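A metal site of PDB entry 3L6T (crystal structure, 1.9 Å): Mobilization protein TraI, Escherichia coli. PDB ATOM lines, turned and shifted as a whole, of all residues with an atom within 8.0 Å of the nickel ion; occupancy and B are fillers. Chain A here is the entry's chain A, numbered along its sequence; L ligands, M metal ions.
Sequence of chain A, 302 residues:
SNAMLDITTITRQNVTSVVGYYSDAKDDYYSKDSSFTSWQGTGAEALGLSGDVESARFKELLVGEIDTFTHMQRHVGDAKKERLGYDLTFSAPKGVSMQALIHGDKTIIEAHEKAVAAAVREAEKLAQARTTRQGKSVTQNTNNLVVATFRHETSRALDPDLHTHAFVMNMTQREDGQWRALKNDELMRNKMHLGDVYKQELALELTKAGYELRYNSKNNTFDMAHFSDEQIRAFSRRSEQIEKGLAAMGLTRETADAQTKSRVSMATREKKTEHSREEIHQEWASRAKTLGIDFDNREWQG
A ring nitrogen (ND1) of His 165 is in hydrogen-bond range of the side-chain hydroxyl (OG1) of Thr 89, 3.2 Å away. The backbone NH of His 165 is in hydrogen-bond range of the backbone carbonyl oxygen of Phe 150 (2.8 Å). The side-chain carboxylate (OD2) of Asp 87 sits at hydrogen-bond distance from a ring nitrogen (ND1) of His 165 (2.7 Å). The side-chain carboxylate (OD1) of Asp 161 is in hydrogen-bond range of a ring nitrogen (ND1) of His 163, at 2.7 Å.
Of the 15 residues printed, 3 come within 4 Å of the nickel ion. The nearest printed residue that does not touch the nickel ion is Val 19 (4.7 Å).
The nickel ion is bound by NE2 of His 165, O6 of the ligand, ND1 of His 152, NE2 of His 163, O3 of the ligand and O5 of the ligand. The nickel ion has six donor atoms within binding distance.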
ATOM      1  N   SER A   1      19.024  -0.169  -5.512  1.00  0.00           N
ATOM      2  CA  SER A   1      18.480   0.464  -4.308  1.00  0.00           C
ATOM      3  C   SER A   1      17.014   0.855  -4.509  1.00  0.00           C
ATOM      4  O   SER A   1      16.391   0.473  -5.501  1.00  0.00           O
ATOM      5  CB  SER A   1      19.291   1.708  -3.937  1.00  0.00           C
ATOM      6  OG  SER A   1      19.101   2.720  -4.906  1.00  0.00           O
ATOM      7  N   VAL A  19      31.648   2.296  -6.158  1.00  0.00           N
ATOM      8  CA  VAL A  19      31.696   0.975  -6.801  1.00  0.00           C
ATOM      9  C   VAL A  19      32.963   0.906  -7.657  1.00  0.00           C
ATOM     10  O   VAL A  19      33.323   1.880  -8.311  1.00  0.00           O
ATOM     11  CB  VAL A  19      30.415   0.669  -7.647  1.00  0.00           C
ATOM     12  CG1 VAL A  19      30.579  -0.621  -8.423  1.00  0.00           C
ATOM     13  CG2 VAL A  19      29.192   0.595  -6.748  1.00  0.00           C
ATOM     14  N   ASP A  87      28.098   8.897  -9.409  1.00  0.00           N
ATOM     15  CA  ASP A  87      27.485   7.594  -9.596  1.00  0.00           C
ATOM     16  C   ASP A  87      25.992   7.799  -9.852  1.00  0.00           C
ATOM     17  O   ASP A  87      25.228   8.127  -8.933  1.00  0.00           O
ATOM     18  CB  ASP A  87      27.696   6.728  -8.360  1.00  0.00           C
ATOM     19  CG  ASP A  87      27.000   5.383  -8.456  1.00  0.00           C
ATOM     20  OD1 ASP A  87      26.226   5.168  -9.419  1.00  0.00           O
ATOM     21  OD2 ASP A  87      27.216   4.543  -7.559  1.00  0.00           O
ATOM     22  N   THR A  89      23.014   5.829 -10.259  1.00  0.00           N
ATOM     23  CA  THR A  89      22.573   4.461 -10.033  1.00  0.00           C
ATOM     24  C   THR A  89      21.106   4.315 -10.458  1.00  0.00           C
ATOM     25  O   THR A  89      20.229   4.906  -9.842  1.00  0.00           O
ATOM     26  CB  THR A  89      22.726   4.053  -8.547  1.00  0.00           C
ATOM     27  OG1 THR A  89      24.058   4.327  -8.098  1.00  0.00           O
ATOM     28  CG2 THR A  89      22.425   2.561  -8.359  1.00  0.00           C
ATOM     29  N   SER A  91      17.948   1.969 -10.728  1.00  0.00           N
ATOM     30  CA  SER A  91      17.362   0.734 -10.199  1.00  0.00           C
ATOM     31  C   SER A  91      16.029   0.371 -10.846  1.00  0.00           C
ATOM     32  O   SER A  91      15.126   1.193 -10.926  1.00  0.00           O
ATOM     33  CB  SER A  91      17.202   0.836  -8.674  1.00  0.00           C
ATOM     34  OG  SER A  91      18.471   1.025  -8.049  1.00  0.00           O
ATOM     35  N   PHE A 150      28.598  -0.602 -13.804  1.00  0.00           N
ATOM     36  CA  PHE A 150      28.717  -1.827 -13.042  1.00  0.00           C
ATOM     37  C   PHE A 150      27.317  -2.323 -12.735  1.00  0.00           C
ATOM     38  O   PHE A 150      26.563  -1.637 -12.040  1.00  0.00           O
ATOM     39  CB  PHE A 150      29.440  -1.567 -11.725  1.00  0.00           C
ATOM     40  CG  PHE A 150      30.813  -1.004 -11.894  1.00  0.00           C
ATOM     41  CD1 PHE A 150      31.932  -1.815 -11.763  1.00  0.00           C
ATOM     42  CD2 PHE A 150      31.003   0.346 -12.176  1.00  0.00           C
ATOM     43  CE1 PHE A 150      33.210  -1.299 -11.902  1.00  0.00           C
ATOM     44  CE2 PHE A 150      32.279   0.871 -12.312  1.00  0.00           C
ATOM     45  CZ  PHE A 150      33.392   0.048 -12.180  1.00  0.00           C
ATOM     46  N   ARG A 151      26.970  -3.511 -13.219  1.00  0.00           N
ATOM     47  CA  ARG A 151      25.671  -4.061 -12.893  1.00  0.00           C
ATOM     48  C   ARG A 151      25.716  -4.868 -11.607  1.00  0.00           C
ATOM     49  O   ARG A 151      26.603  -5.707 -11.419  1.00  0.00           O
ATOM     50  CB  ARG A 151      25.108  -4.934 -14.029  1.00  0.00           C
ATOM     51  CG  ARG A 151      23.715  -5.485 -13.678  1.00  0.00           C
ATOM     52  CD  ARG A 151      23.067  -6.163 -14.848  1.00  0.00           C
ATOM     53  NE  ARG A 151      23.722  -7.416 -15.187  1.00  0.00           N
ATOM     54  CZ  ARG A 151      24.506  -7.574 -16.244  1.00  0.00           C
ATOM     55  NH1 ARG A 151      25.071  -8.756 -16.478  1.00  0.00           N
ATOM     56  NH2 ARG A 151      24.721  -6.556 -17.056  1.00  0.00           N
ATOM     57  N   HIS A 152      24.771  -4.598 -10.731  1.00  0.00           N
ATOM     58  CA  HIS A 152      24.620  -5.363  -9.507  1.00  0.00           C
ATOM     59  C   HIS A 152      23.328  -6.171  -9.518  1.00  0.00           C
ATOM     60  O   HIS A 152      22.242  -5.641  -9.762  1.00  0.00           O
ATOM     61  CB  HIS A 152      24.686  -4.447  -8.291  1.00  0.00           C
ATOM     62  CG  HIS A 152      26.074  -3.935  -8.021  1.00  0.00           C
ATOM     63  ND1 HIS A 152      26.343  -2.937  -7.121  1.00  0.00           N
ATOM     64  CD2 HIS A 152      27.270  -4.289  -8.563  1.00  0.00           C
ATOM     65  CE1 HIS A 152      27.644  -2.696  -7.095  1.00  0.00           C
ATOM     66  NE2 HIS A 152      28.225  -3.515  -7.964  1.00  0.00           N
ATOM     67  N   GLU A 153      23.465  -7.468  -9.291  1.00  0.00           N
ATOM     68  CA  GLU A 153      22.313  -8.356  -9.274  1.00  0.00           C
ATOM     69  C   GLU A 153      22.152  -8.911  -7.870  1.00  0.00           C
ATOM     70  O   GLU A 153      22.787  -9.910  -7.502  1.00  0.00           O
ATOM     71  CB  GLU A 153      22.474  -9.457 -10.333  1.00  0.00           C
ATOM     72  CG  GLU A 153      22.580  -8.917 -11.768  1.00  0.00           C
ATOM     73  CD  GLU A 153      22.725 -10.011 -12.830  1.00  0.00           C
ATOM     74  OE1 GLU A 153      22.575 -11.204 -12.494  1.00  0.00           O
ATOM     75  OE2 GLU A 153      22.992  -9.673 -14.009  1.00  0.00           O
ATOM     76  N   THR A 154      21.337  -8.244  -7.067  1.00  0.00           N
ATOM     77  CA  THR A 154      21.048  -8.701  -5.704  1.00  0.00           C
ATOM     78  C   THR A 154      19.935  -9.729  -5.756  1.00  0.00           C
ATOM     79  O   THR A 154      18.762  -9.370  -5.612  1.00  0.00           O
ATOM     80  CB  THR A 154      20.615  -7.551  -4.793  1.00  0.00           C
ATOM     81  OG1 THR A 154      21.563  -6.484  -4.866  1.00  0.00           O
ATOM     82  CG2 THR A 154      20.498  -8.046  -3.366  1.00  0.00           C
ATOM     83  N   ASP A 161      16.847  -6.952  -6.246  1.00  0.00           N
ATOM     84  CA  ASP A 161      17.169  -5.594  -6.674  1.00  0.00           C
ATOM     85  C   ASP A 161      18.149  -5.639  -7.845  1.00  0.00           C
ATOM     86  O   ASP A 161      19.305  -6.004  -7.685  1.00  0.00           O
ATOM     87  CB  ASP A 161      17.787  -4.815  -5.504  1.00  0.00           C
ATOM     88  CG  ASP A 161      18.060  -3.358  -5.843  1.00  0.00           C
ATOM     89  OD1 ASP A 161      18.482  -3.060  -6.973  1.00  0.00           O
ATOM     90  OD2 ASP A 161      17.842  -2.499  -4.958  1.00  0.00           O
ATOM     91  N   LEU A 162      17.654  -5.303  -9.033  1.00  0.00           N
ATOM     92  CA  LEU A 162      18.510  -5.156 -10.197  1.00  0.00           C
ATOM     93  C   LEU A 162      18.812  -3.682 -10.399  1.00  0.00           C
ATOM     94  O   LEU A 162      17.908  -2.854 -10.501  1.00  0.00           O
ATOM     95  CB  LEU A 162      17.824  -5.720 -11.452  1.00  0.00           C
ATOM     96  CG  LEU A 162      18.476  -5.363 -12.802  1.00  0.00           C
ATOM     97  CD1 LEU A 162      19.811  -6.075 -12.992  1.00  0.00           C
ATOM     98  CD2 LEU A 162      17.521  -5.699 -13.946  1.00  0.00           C
ATOM     99  N   HIS A 163      20.089  -3.348 -10.446  1.00  0.00           N
ATOM    100  CA  HIS A 163      20.475  -1.972 -10.710  1.00  0.00           C
ATOM    101  C   HIS A 163      21.849  -1.898 -11.344  1.00  0.00           C
ATOM    102  O   HIS A 163      22.622  -2.855 -11.290  1.00  0.00           O
ATOM    103  CB  HIS A 163      20.452  -1.141  -9.406  1.00  0.00           C
ATOM    104  CG  HIS A 163      21.416  -1.614  -8.371  1.00  0.00           C
ATOM    105  ND1 HIS A 163      21.102  -2.595  -7.456  1.00  0.00           N
ATOM    106  CD2 HIS A 163      22.676  -1.221  -8.079  1.00  0.00           C
ATOM    107  CE1 HIS A 163      22.135  -2.793  -6.644  1.00  0.00           C
ATOM    108  NE2 HIS A 163      23.094  -1.959  -6.994  1.00  0.00           N
ATOM    109  N   THR A 164      22.134  -0.753 -11.952  1.00  0.00           N
ATOM    110  CA  THR A 164      23.438  -0.535 -12.557  1.00  0.00           C
ATOM    111  C   THR A 164      23.989   0.792 -12.060  1.00  0.00           C
ATOM    112  O   THR A 164      23.275   1.811 -12.054  1.00  0.00           O
ATOM    113  CB  THR A 164      23.362  -0.542 -14.103  1.00  0.00           C
ATOM    114  OG1 THR A 164      23.050  -1.877 -14.541  1.00  0.00           O
ATOM    115  CG2 THR A 164      24.686  -0.131 -14.717  1.00  0.00           C
ATOM    116  N   HIS A 165      25.238   0.769 -11.601  1.00  0.00           N
ATOM    117  CA  HIS A 165      25.939   2.001 -11.255  1.00  0.00           C
ATOM    118  C   HIS A 165      26.611   2.527 -12.505  1.00  0.00           C
ATOM    119  O   HIS A 165      27.530   1.891 -13.014  1.00  0.00           O
ATOM    120  CB  HIS A 165      27.011   1.720 -10.217  1.00  0.00           C
ATOM    121  CG  HIS A 165      26.478   1.217  -8.920  1.00  0.00           C
ATOM    122  ND1 HIS A 165      26.273   2.036  -7.833  1.00  0.00           N
ATOM    123  CD2 HIS A 165      26.116  -0.030  -8.531  1.00  0.00           C
ATOM    124  CE1 HIS A 165      25.807   1.320  -6.826  1.00  0.00           C
ATOM    125  NE2 HIS A 165      25.699   0.063  -7.230  1.00  0.00           N
HETATM  126  C1  LIG L   1      21.764  -0.467  -3.077  1.00  0.00           C
HETATM  127  O1  LIG L   1      21.617  -0.685  -4.237  1.00  0.00           O
HETATM  128  O2  LIG L   1      20.681  -0.633  -2.211  1.00  0.00           O
HETATM  129  C2  LIG L   1      23.140  -0.127  -2.490  1.00  0.00           C
HETATM  130  C3  LIG L   1      24.307  -0.597  -3.369  1.00  0.00           C
HETATM  131  O3  LIG L   1      24.052  -0.160  -4.661  1.00  0.00           O
HETATM  132  C4  LIG L   1      25.635  -0.023  -2.908  1.00  0.00           C
HETATM  133  C5  LIG L   1      26.837  -0.276  -3.821  1.00  0.00           C
HETATM  134  O4  LIG L   1      28.064   0.278  -3.450  1.00  0.00           O
HETATM  135  O5  LIG L   1      26.849  -1.224  -4.538  1.00  0.00           O
HETATM  136  C6  LIG L   1      24.390  -2.120  -3.293  1.00  0.00           C
HETATM  137  O6  LIG L   1      24.445  -2.887  -4.464  1.00  0.00           O
HETATM  138  O7  LIG L   1      24.279  -2.672  -2.256  1.00  0.00           O
HETATM  139 NI    NI M   1      25.043  -1.572  -6.066  1.00  0.00          NI
